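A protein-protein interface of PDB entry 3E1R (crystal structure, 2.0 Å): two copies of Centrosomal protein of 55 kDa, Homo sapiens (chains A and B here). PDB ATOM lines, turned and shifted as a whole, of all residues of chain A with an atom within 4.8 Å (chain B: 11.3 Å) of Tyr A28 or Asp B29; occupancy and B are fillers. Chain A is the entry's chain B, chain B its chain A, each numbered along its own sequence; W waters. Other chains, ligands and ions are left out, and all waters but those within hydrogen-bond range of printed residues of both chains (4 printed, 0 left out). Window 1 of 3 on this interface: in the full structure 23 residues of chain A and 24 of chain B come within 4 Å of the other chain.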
ATOM      1  N   GLN A  24      23.938 -19.193 -26.546  1.00  0.00           N
ATOM      2  CA  GLN A  24      25.150 -19.782 -27.111  1.00  0.00           C
ATOM      3  C   GLN A  24      25.558 -21.000 -26.289  1.00  0.00           C
ATOM      4  O   GLN A  24      26.023 -22.003 -26.837  1.00  0.00           O
ATOM      5  CB  GLN A  24      26.296 -18.768 -27.133  1.00  0.00           C
ATOM      6  CG  GLN A  24      26.247 -17.788 -28.302  1.00  0.00           C
ATOM      7  CD  GLN A  24      27.356 -16.756 -28.234  1.00  0.00           C
ATOM      8  OE1 GLN A  24      27.498 -16.050 -27.237  1.00  0.00           O
ATOM      9  NE2 GLN A  24      28.145 -16.661 -29.297  1.00  0.00           N
ATOM     10  N   TRP A  25      25.392 -20.920 -24.971  1.00  0.00           N
ATOM     11  CA  TRP A  25      25.739 -22.053 -24.124  1.00  0.00           C
ATOM     12  C   TRP A  25      24.927 -23.289 -24.487  1.00  0.00           C
ATOM     13  O   TRP A  25      25.450 -24.400 -24.514  1.00  0.00           O
ATOM     14  CB  TRP A  25      25.529 -21.714 -22.641  1.00  0.00           C
ATOM     15  CG  TRP A  25      26.736 -21.124 -21.979  1.00  0.00           C
ATOM     16  CD1 TRP A  25      26.852 -19.874 -21.453  1.00  0.00           C
ATOM     17  CD2 TRP A  25      27.999 -21.771 -21.761  1.00  0.00           C
ATOM     18  NE1 TRP A  25      28.110 -19.694 -20.927  1.00  0.00           N
ATOM     19  CE2 TRP A  25      28.838 -20.839 -21.113  1.00  0.00           C
ATOM     20  CE3 TRP A  25      28.510 -23.039 -22.076  1.00  0.00           C
ATOM     21  CZ2 TRP A  25      30.152 -21.144 -20.743  1.00  0.00           C
ATOM     22  CZ3 TRP A  25      29.824 -23.340 -21.708  1.00  0.00           C
ATOM     23  CH2 TRP A  25      30.629 -22.391 -21.059  1.00  0.00           C
ATOM     24  N   LEU A  26      23.646 -23.089 -24.779  1.00  0.00           N
ATOM     25  CA  LEU A  26      22.754 -24.195 -25.133  1.00  0.00           C
ATOM     26  C   LEU A  26      23.196 -24.898 -26.407  1.00  0.00           C
ATOM     27  O   LEU A  26      23.193 -26.118 -26.491  1.00  0.00           O
ATOM     28  CB  LEU A  26      21.324 -23.690 -25.316  1.00  0.00           C
ATOM     29  CG  LEU A  26      20.436 -23.570 -24.077  1.00  0.00           C
ATOM     30  CD1 LEU A  26      21.235 -23.063 -22.890  1.00  0.00           C
ATOM     31  CD2 LEU A  26      19.272 -22.646 -24.387  1.00  0.00           C
ATOM     32  N   VAL A  27      23.569 -24.098 -27.396  1.00  0.00           N
ATOM     33  CA  VAL A  27      24.029 -24.604 -28.678  1.00  0.00           C
ATOM     34  C   VAL A  27      25.325 -25.371 -28.496  1.00  0.00           C
ATOM     35  O   VAL A  27      25.467 -26.494 -28.973  1.00  0.00           O
ATOM     36  CB  VAL A  27      24.245 -23.426 -29.659  1.00  0.00           C
ATOM     37  CG1 VAL A  27      24.923 -23.922 -30.926  1.00  0.00           C
ATOM     38  CG2 VAL A  27      22.913 -22.776 -29.975  1.00  0.00           C
ATOM     39  N   TYR A  28      26.261 -24.753 -27.789  1.00  0.00           N
ATOM     40  CA  TYR A  28      27.560 -25.360 -27.521  1.00  0.00           C
ATOM     41  C   TYR A  28      27.426 -26.661 -26.738  1.00  0.00           C
ATOM     42  O   TYR A  28      28.070 -27.659 -27.056  1.00  0.00           O
ATOM     43  CB  TYR A  28      28.440 -24.394 -26.735  1.00  0.00           C
ATOM     44  CG  TYR A  28      29.828 -24.911 -26.441  1.00  0.00           C
ATOM     45  CD1 TYR A  28      30.234 -25.179 -25.134  1.00  0.00           C
ATOM     46  CD2 TYR A  28      30.754 -25.088 -27.464  1.00  0.00           C
ATOM     47  CE1 TYR A  28      31.537 -25.603 -24.853  1.00  0.00           C
ATOM     48  CE2 TYR A  28      32.060 -25.515 -27.199  1.00  0.00           C
ATOM     49  CZ  TYR A  28      32.444 -25.766 -25.894  1.00  0.00           C
ATOM     50  OH  TYR A  28      33.734 -26.164 -25.623  1.00  0.00           O
ATOM     51  N   ASP A  29      26.590 -26.649 -25.708  1.00  0.00           N
ATOM     52  CA  ASP A  29      26.393 -27.838 -24.891  1.00  0.00           C
ATOM     53  C   ASP A  29      25.966 -29.060 -25.703  1.00  0.00           C
ATOM     54  O   ASP A  29      26.547 -30.132 -25.561  1.00  0.00           O
ATOM     55  CB  ASP A  29      25.356 -27.574 -23.799  1.00  0.00           C
ATOM     56  CG  ASP A  29      25.071 -28.811 -22.968  1.00  0.00           C
ATOM     57  OD1 ASP A  29      25.970 -29.244 -22.224  1.00  0.00           O
ATOM     58  OD2 ASP A  29      23.951 -29.352 -23.067  1.00  0.00           O
ATOM     59  N   GLN A  30      24.963 -28.915 -26.566  1.00  0.00           N
ATOM     60  CA  GLN A  30      24.520 -30.074 -27.332  1.00  0.00           C
ATOM     61  C   GLN A  30      25.621 -30.575 -28.261  1.00  0.00           C
ATOM     62  O   GLN A  30      25.724 -31.781 -28.505  1.00  0.00           O
ATOM     63  CB  GLN A  30      23.188 -29.775 -28.061  1.00  0.00           C
ATOM     64  CG  GLN A  30      23.191 -29.664 -29.578  1.00  0.00           C
ATOM     65  CD  GLN A  30      23.502 -30.962 -30.297  1.00  0.00           C
ATOM     66  OE1 GLN A  30      23.003 -32.032 -29.938  1.00  0.00           O
ATOM     67  NE2 GLN A  30      24.322 -30.870 -31.338  1.00  0.00           N
ATOM     68  N   GLN A  31      26.463 -29.664 -28.746  1.00  0.00           N
ATOM     69  CA  GLN A  31      27.588 -30.038 -29.599  1.00  0.00           C
ATOM     70  C   GLN A  31      28.593 -30.810 -28.738  1.00  0.00           C
ATOM     71  O   GLN A  31      29.060 -31.883 -29.119  1.00  0.00           O
ATOM     72  CB  GLN A  31      28.274 -28.791 -30.185  1.00  0.00           C
ATOM     73  CG  GLN A  31      27.639 -28.232 -31.454  1.00  0.00           C
ATOM     74  CD  GLN A  31      28.248 -26.898 -31.881  1.00  0.00           C
ATOM     75  OE1 GLN A  31      29.318 -26.508 -31.408  1.00  0.00           O
ATOM     76  NE2 GLN A  31      27.567 -26.198 -32.785  1.00  0.00           N
ATOM     77  N   ARG A  32      28.917 -30.263 -27.570  1.00  0.00           N
ATOM     78  CA  ARG A  32      29.864 -30.922 -26.681  1.00  0.00           C
ATOM     79  C   ARG A  32      29.399 -32.296 -26.221  1.00  0.00           C
ATOM     80  O   ARG A  32      30.206 -33.216 -26.088  1.00  0.00           O
ATOM     81  CB  ARG A  32      30.169 -30.057 -25.450  1.00  0.00           C
ATOM     82  CG  ARG A  32      31.098 -28.894 -25.734  1.00  0.00           C
ATOM     83  CD  ARG A  32      32.298 -29.330 -26.584  1.00  0.00           C
ATOM     84  NE  ARG A  32      33.467 -29.744 -25.811  1.00  0.00           N
ATOM     85  CZ  ARG A  32      34.572 -30.243 -26.355  1.00  0.00           C
ATOM     86  NH1 ARG A  32      34.652 -30.404 -27.671  1.00  0.00           N
ATOM     87  NH2 ARG A  32      35.610 -30.563 -25.594  1.00  0.00           N
ATOM     88  N   GLU B  20      23.523 -15.637 -13.476  1.00  0.00           N
ATOM     89  CA  GLU B  20      23.645 -16.821 -12.645  1.00  0.00           C
ATOM     90  C   GLU B  20      23.676 -18.074 -13.513  1.00  0.00           C
ATOM     91  O   GLU B  20      24.519 -18.945 -13.324  1.00  0.00           O
ATOM     92  CB  GLU B  20      22.480 -16.896 -11.657  1.00  0.00           C
ATOM     93  CG  GLU B  20      22.364 -18.228 -10.936  1.00  0.00           C
ATOM     94  CD  GLU B  20      21.324 -18.206  -9.832  1.00  0.00           C
ATOM     95  OE1 GLU B  20      21.628 -17.678  -8.741  1.00  0.00           O
ATOM     96  OE2 GLU B  20      20.200 -18.707 -10.059  1.00  0.00           O
ATOM     97  N   LYS B  21      22.763 -18.159 -14.473  1.00  0.00           N
ATOM     98  CA  LYS B  21      22.711 -19.324 -15.342  1.00  0.00           C
ATOM     99  C   LYS B  21      23.960 -19.476 -16.217  1.00  0.00           C
ATOM    100  O   LYS B  21      24.424 -20.594 -16.444  1.00  0.00           O
ATOM    101  CB  LYS B  21      21.422 -19.285 -16.168  1.00  0.00           C
ATOM    102  CG  LYS B  21      20.213 -19.732 -15.343  1.00  0.00           C
ATOM    103  CD  LYS B  21      18.884 -19.356 -15.963  1.00  0.00           C
ATOM    104  CE  LYS B  21      17.730 -20.025 -15.218  1.00  0.00           C
ATOM    105  NZ  LYS B  21      17.805 -19.831 -13.741  1.00  0.00           N
ATOM    106  N   ASN B  22      24.521 -18.364 -16.685  1.00  0.00           N
ATOM    107  CA  ASN B  22      25.734 -18.433 -17.497  1.00  0.00           C
ATOM    108  C   ASN B  22      26.923 -18.871 -16.644  1.00  0.00           C
ATOM    109  O   ASN B  22      27.801 -19.582 -17.124  1.00  0.00           O
ATOM    110  CB  ASN B  22      26.041 -17.085 -18.156  1.00  0.00           C
ATOM    111  CG  ASN B  22      25.053 -16.732 -19.252  1.00  0.00           C
ATOM    112  OD1 ASN B  22      24.319 -17.591 -19.738  1.00  0.00           O
ATOM    113  ND2 ASN B  22      25.046 -15.465 -19.657  1.00  0.00           N
ATOM    114  N   GLN B  23      26.950 -18.452 -15.380  1.00  0.00           N
ATOM    115  CA  GLN B  23      28.030 -18.839 -14.474  1.00  0.00           C
ATOM    116  C   GLN B  23      27.910 -20.332 -14.155  1.00  0.00           C
ATOM    117  O   GLN B  23      28.914 -21.033 -13.996  1.00  0.00           O
ATOM    118  CB  GLN B  23      27.965 -18.020 -13.183  1.00  0.00           C
ATOM    119  CG  GLN B  23      29.019 -18.384 -12.137  1.00  0.00           C
ATOM    120  CD  GLN B  23      30.441 -18.223 -12.646  1.00  0.00           C
ATOM    121  OE1 GLN B  23      30.687 -17.530 -13.636  1.00  0.00           O
ATOM    122  NE2 GLN B  23      31.391 -18.853 -11.957  1.00  0.00           N
ATOM    123  N   GLN B  24      26.672 -20.810 -14.049  1.00  0.00           N
ATOM    124  CA  GLN B  24      26.427 -22.223 -13.780  1.00  0.00           C
ATOM    125  C   GLN B  24      26.907 -23.033 -14.990  1.00  0.00           C
ATOM    126  O   GLN B  24      27.523 -24.087 -14.833  1.00  0.00           O
ATOM    127  CB  GLN B  24      24.934 -22.488 -13.557  1.00  0.00           C
ATOM    128  CG  GLN B  24      24.331 -21.818 -12.326  1.00  0.00           C
ATOM    129  CD  GLN B  24      22.823 -21.976 -12.266  1.00  0.00           C
ATOM    130  OE1 GLN B  24      22.160 -22.089 -13.297  1.00  0.00           O
ATOM    131  NE2 GLN B  24      22.268 -21.967 -11.059  1.00  0.00           N
ATOM    132  N   TRP B  25      26.619 -22.536 -16.192  1.00  0.00           N
ATOM    133  CA  TRP B  25      27.039 -23.226 -17.410  1.00  0.00           C
ATOM    134  C   TRP B  25      28.560 -23.323 -17.459  1.00  0.00           C
ATOM    135  O   TRP B  25      29.108 -24.353 -17.848  1.00  0.00           O
ATOM    136  CB  TRP B  25      26.531 -22.501 -18.667  1.00  0.00           C
ATOM    137  CG  TRP B  25      25.207 -22.993 -19.193  1.00  0.00           C
ATOM    138  CD1 TRP B  25      24.036 -22.291 -19.252  1.00  0.00           C
ATOM    139  CD2 TRP B  25      24.925 -24.288 -19.748  1.00  0.00           C
ATOM    140  NE1 TRP B  25      23.047 -23.066 -19.811  1.00  0.00           N
ATOM    141  CE2 TRP B  25      23.565 -24.294 -20.125  1.00  0.00           C
ATOM    142  CE3 TRP B  25      25.694 -25.441 -19.966  1.00  0.00           C
ATOM    143  CZ2 TRP B  25      22.951 -25.413 -20.706  1.00  0.00           C
ATOM    144  CZ3 TRP B  25      25.086 -26.550 -20.543  1.00  0.00           C
ATOM    145  CH2 TRP B  25      23.726 -26.527 -20.908  1.00  0.00           C
ATOM    146  N   LEU B  26      29.236 -22.250 -17.056  1.00  0.00           N
ATOM    147  CA  LEU B  26      30.695 -22.223 -17.065  1.00  0.00           C
ATOM    148  C   LEU B  26      31.269 -23.262 -16.114  1.00  0.00           C
ATOM    149  O   LEU B  26      32.229 -23.947 -16.446  1.00  0.00           O
ATOM    150  CB  LEU B  26      31.217 -20.838 -16.668  1.00  0.00           C
ATOM    151  CG  LEU B  26      32.747 -20.710 -16.640  1.00  0.00           C
ATOM    152  CD1 LEU B  26      33.288 -20.748 -18.065  1.00  0.00           C
ATOM    153  CD2 LEU B  26      33.150 -19.414 -15.955  1.00  0.00           C
ATOM    154  N   VAL B  27      30.689 -23.359 -14.923  1.00  0.00           N
ATOM    155  CA  VAL B  27      31.140 -24.329 -13.928  1.00  0.00           C
ATOM    156  C   VAL B  27      30.957 -25.745 -14.484  1.00  0.00           C
ATOM    157  O   VAL B  27      31.859 -26.580 -14.425  1.00  0.00           O
ATOM    158  CB  VAL B  27      30.336 -24.176 -12.611  1.00  0.00           C
ATOM    159  CG1 VAL B  27      30.464 -25.431 -11.764  1.00  0.00           C
ATOM    160  CG2 VAL B  27      30.844 -22.971 -11.830  1.00  0.00           C
ATOM    161  N   TYR B  28      29.774 -25.995 -15.027  1.00  0.00           N
ATOM    162  CA  TYR B  28      29.421 -27.279 -15.612  1.00  0.00           C
ATOM    163  C   TYR B  28      30.384 -27.649 -16.740  1.00  0.00           C
ATOM    164  O   TYR B  28      30.930 -28.751 -16.767  1.00  0.00           O
ATOM    165  CB  TYR B  28      27.986 -27.194 -16.126  1.00  0.00           C
ATOM    166  CG  TYR B  28      27.398 -28.452 -16.716  1.00  0.00           C
ATOM    167  CD1 TYR B  28      27.321 -28.622 -18.099  1.00  0.00           C
ATOM    168  CD2 TYR B  28      26.827 -29.429 -15.899  1.00  0.00           C
ATOM    169  CE1 TYR B  28      26.675 -29.730 -18.658  1.00  0.00           C
ATOM    170  CE2 TYR B  28      26.180 -30.538 -16.447  1.00  0.00           C
ATOM    171  CZ  TYR B  28      26.106 -30.677 -17.827  1.00  0.00           C
ATOM    172  OH  TYR B  28      25.418 -31.733 -18.374  1.00  0.00           O
ATOM    173  N   ASP B  29      30.609 -26.717 -17.660  1.00  0.00           N
ATOM    174  CA  ASP B  29      31.507 -26.959 -18.786  1.00  0.00           C
ATOM    175  C   ASP B  29      32.955 -27.186 -18.347  1.00  0.00           C
ATOM    176  O   ASP B  29      33.665 -28.005 -18.935  1.00  0.00           O
ATOM    177  CB  ASP B  29      31.437 -25.796 -19.778  1.00  0.00           C
ATOM    178  CG  ASP B  29      32.199 -26.080 -21.055  1.00  0.00           C
ATOM    179  OD1 ASP B  29      31.751 -26.942 -21.840  1.00  0.00           O
ATOM    180  OD2 ASP B  29      33.253 -25.449 -21.268  1.00  0.00           O
ATOM    181  N   GLN B  30      33.404 -26.466 -17.323  1.00  0.00           N
ATOM    182  CA  GLN B  30      34.770 -26.643 -16.834  1.00  0.00           C
ATOM    183  C   GLN B  30      34.929 -28.057 -16.280  1.00  0.00           C
ATOM    184  O   GLN B  30      35.963 -28.697 -16.473  1.00  0.00           O
ATOM    185  CB  GLN B  30      35.101 -25.605 -15.751  1.00  0.00           C
ATOM    186  CG  GLN B  30      35.339 -24.192 -16.291  1.00  0.00           C
ATOM    187  CD  GLN B  30      35.464 -23.134 -15.194  1.00  0.00           C
ATOM    188  OE1 GLN B  30      35.097 -23.368 -14.039  1.00  0.00           O
ATOM    189  NE2 GLN B  30      35.960 -21.954 -15.562  1.00  0.00           N
ATOM    190  N   GLN B  31      33.902 -28.544 -15.591  1.00  0.00           N
ATOM    191  CA  GLN B  31      33.938 -29.889 -15.036  1.00  0.00           C
ATOM    192  C   GLN B  31      33.926 -30.906 -16.180  1.00  0.00           C
ATOM    193  O   GLN B  31      34.611 -31.926 -16.113  1.00  0.00           O
ATOM    194  CB  GLN B  31      32.758 -30.090 -14.078  1.00  0.00           C
ATOM    195  CG  GLN B  31      32.842 -29.163 -12.856  1.00  0.00           C
ATOM    196  CD  GLN B  31      31.578 -29.132 -12.015  1.00  0.00           C
ATOM    197  OE1 GLN B  31      30.525 -29.609 -12.440  1.00  0.00           O
ATOM    198  NE2 GLN B  31      31.675 -28.551 -10.821  1.00  0.00           N
ATOM    199  N   ARG B  32      33.160 -30.632 -17.231  1.00  0.00           N
ATOM    200  CA  ARG B  32      33.128 -31.527 -18.386  1.00  0.00           C
ATOM    201  C   ARG B  32      34.526 -31.602 -18.996  1.00  0.00           C
ATOM    202  O   ARG B  32      34.992 -32.675 -19.380  1.00  0.00           O
ATOM    203  CB  ARG B  32      32.144 -31.020 -19.450  1.00  0.00           C
ATOM    204  CG  ARG B  32      32.221 -31.801 -20.772  1.00  0.00           C
ATOM    205  CD  ARG B  32      31.006 -31.544 -21.649  1.00  0.00           C
ATOM    206  NE  ARG B  32      30.756 -30.115 -21.797  1.00  0.00           N
ATOM    207  CZ  ARG B  32      29.559 -29.586 -22.015  1.00  0.00           C
ATOM    208  NH1 ARG B  32      28.489 -30.367 -22.113  1.00  0.00           N
ATOM    209  NH2 ARG B  32      29.432 -28.270 -22.118  1.00  0.00           N
ATOM    210  N   GLU B  33      35.198 -30.460 -19.091  1.00  0.00           N
ATOM    211  CA  GLU B  33      36.545 -30.439 -19.655  1.00  0.00           C
ATOM    212  C   GLU B  33      37.504 -31.313 -18.841  1.00  0.00           C
ATOM    213  O   GLU B  33      38.368 -31.988 -19.394  1.00  0.00           O
ATOM    214  CB  GLU B  33      37.054 -29.002 -19.754  1.00  0.00           C
ATOM    215  CG  GLU B  33      36.445 -28.244 -20.925  1.00  0.00           C
ATOM    216  CD  GLU B  33      36.709 -28.943 -22.256  1.00  0.00           C
ATOM    217  OE1 GLU B  33      37.891 -29.162 -22.584  1.00  0.00           O
ATOM    218  OE2 GLU B  33      35.742 -29.276 -22.975  1.00  0.00           O
ATOM    219  N   VAL B  34      37.350 -31.311 -17.525  1.00  0.00           N
ATOM    220  CA  VAL B  34      38.196 -32.148 -16.686  1.00  0.00           C
ATOM    221  C   VAL B  34      37.872 -33.616 -17.015  1.00  0.00           C
ATOM    222  O   VAL B  34      38.768 -34.431 -17.226  1.00  0.00           O
ATOM    223  CB  VAL B  34      37.942 -31.866 -15.181  1.00  0.00           C
ATOM    224  CG1 VAL B  34      38.555 -32.966 -14.332  1.00  0.00           C
ATOM    225  CG2 VAL B  34      38.543 -30.507 -14.791  1.00  0.00           C
ATOM    226  N   TYR B  35      36.582 -33.931 -17.073  1.00  0.00           N
ATOM    227  CA  TYR B  35      36.092 -35.281 -17.388  1.00  0.00           C
ATOM    228  C   TYR B  35      36.621 -35.738 -18.749  1.00  0.00           C
ATOM    229  O   TYR B  35      37.019 -36.893 -18.915  1.00  0.00           O
ATOM    230  CB  TYR B  35      34.559 -35.268 -17.401  1.00  0.00           C
ATOM    231  CG  TYR B  35      33.866 -36.590 -17.685  1.00  0.00           C
ATOM    232  CD1 TYR B  35      33.863 -37.623 -16.737  1.00  0.00           C
ATOM    233  CD2 TYR B  35      33.160 -36.783 -18.875  1.00  0.00           C
ATOM    234  CE1 TYR B  35      33.162 -38.815 -16.970  1.00  0.00           C
ATOM    235  CE2 TYR B  35      32.460 -37.964 -19.116  1.00  0.00           C
ATOM    236  CZ  TYR B  35      32.462 -38.972 -18.164  1.00  0.00           C
ATOM    237  OH  TYR B  35      31.764 -40.131 -18.410  1.00  0.00           O
ATOM    238  N   VAL B  36      36.619 -34.828 -19.715  1.00  0.00           N
ATOM    239  CA  VAL B  36      37.103 -35.135 -21.064  1.00  0.00           C
ATOM    240  C   VAL B  36      38.585 -35.499 -21.063  1.00  0.00           C
ATOM    241  O   VAL B  36      39.000 -36.417 -21.772  1.00  0.00           O
ATOM    242  CB  VAL B  36      36.859 -33.948 -22.032  1.00  0.00           C
ATOM    243  CG1 VAL B  36      37.646 -34.138 -23.328  1.00  0.00           C
ATOM    244  CG2 VAL B  36      35.375 -33.847 -22.344  1.00  0.00           C
ATOM    245  N   LYS B  37      39.382 -34.789 -20.271  1.00  0.00           N
ATOM    246  CA  LYS B  37      40.800 -35.102 -20.203  1.00  0.00           C
ATOM    247  C   LYS B  37      40.953 -36.547 -19.727  1.00  0.00           C
ATOM    248  O   LYS B  37      41.811 -37.276 -20.212  1.00  0.00           O
ATOM    249  CB  LYS B  37      41.519 -34.112 -19.270  1.00  0.00           C
ATOM    250  CG  LYS B  37      41.695 -32.735 -19.916  1.00  0.00           C
ATOM    251  CD  LYS B  37      42.274 -31.680 -18.978  1.00  0.00           C
ATOM    252  CE  LYS B  37      42.485 -30.344 -19.706  1.00  0.00           C
ATOM    253  NZ  LYS B  37      41.228 -29.733 -20.239  1.00  0.00           N
ATOM    254  N   GLY B  38      40.089 -36.958 -18.798  1.00  0.00           N
ATOM    255  CA  GLY B  38      40.128 -38.317 -18.290  1.00  0.00           C
ATOM    256  C   GLY B  38      39.767 -39.331 -19.366  1.00  0.00           C
ATOM    257  O   GLY B  38      40.382 -40.391 -19.456  1.00  0.00           O
HETATM  258  O   HOH W   1      33.179 -28.731 -22.836  1.00  0.00           O
HETATM  259  O   HOH W   2      34.964 -25.761 -23.276  1.00  0.00           O
HETATM  260  O   HOH W   3      24.850 -31.392 -21.036  1.00  0.00           O
HETATM  261  O   HOH W   4      29.308 -17.951 -18.841  1.00  0.00           O
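Water W1 lies within hydrogen-bond range of OD1 of Asp B29 (2.5 Å), OE2 of Glu B33 (2.6 Å), NE of Arg B32 (3.0 Å) and NE of Arg A32 (3.2 Å).
Water W2 lies within hydrogen-bond range of the side-chain carboxylate (OD2) of Asp B29 (2.7 Å) and the side-chain hydroxyl (OH) of Tyr A28 (2.7 Å).
Water W3 lies within hydrogen-bond range of OD1 of Asp A29 and OH of Tyr B28.
Water W4 lies within hydrogen-bond range of O of Asn B22 (2.8 Å) and NE1 of Trp A25 (3.0 Å).
Trp A25 touches Leu B26, and with the chains exchanged Leu A26 touches Trp B25.
Trp A25 touches Asp B29, and with the chains exchanged Asp A29 touches Trp B25.
Tyr A28 touches Asp B29, and with the chains exchanged Asp A29 touches Tyr B28.
Arg A32 touches its own counterpart, Arg B32.
Of the 11 pairs that touch across the chains among the printed residues, 8 have their exchanged pair printed and touching as well.
Of the printed residues of chain B, Trp A25 touches Asn B22, Trp B25, Leu B26 and Asp B29.
No residue of chain B comes within 4 Å of Val A27.
Tyr A28 touches just one residue of chain B: Asp B29.
Printed residues of chain B within 4 Å of Asp A29: Trp B25 (3.3 Å), Tyr B28 (3.7 Å) and Arg B32 (2.8 Å).
Gln A30 touches none of the printed residues of chain B.
Printed residues of chain A within 4 Å of Asn B22: Trp A25 (3.8 Å).
Of the printed residues of chain A, Leu B26 touches Trp A25.
Of chain A, only Trp A25 and Tyr A28 come within 4 Å of Asp B29.
Printed residues of chain A within 4 Å of Glu B33: Arg A32.
The nearest residue of chain A that does not touch Asp B29 is Arg A32 (4.4 Å).
Of the 9 printed residues of chain A, 5 touch a printed residue of chain B.
Printed residues of chain A that touch a printed residue of chain B: Trp A25, Leu A26, Tyr A28, Asp A29 and Arg A32.
Printed residues of chain B that touch a printed residue of chain A: Asn B22, Trp B25, Leu B26, Tyr B28, Asp B29, Arg B32 and Glu B33.
Hydrophobic or aromatic side chains of chain B that line the printed part of chain A: Trp B25 and Tyr B28.
NH2 of Arg A32 is in salt-bridge range of OE2 of Glu B33 (2.9 Å).
NH1 of Arg B32 lies within salt-bridge range of OD1 of Asp A29, at 2.8 Å.
Among the printed residues, pairs that only touch across the chains: Asp A29 with Trp B25, Tyr A28 with Asp B29, Trp A25 with Trp B25, Trp A25 with Asp B29, Arg A32 with Arg B32, Leu A26 with Trp B25, Asp A29 with Tyr B28, Trp A25 with Asn B22 and Trp A25 with Leu B26.
OD1 of Asp B29 is in salt-bridge range of NH2 of Arg B32.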
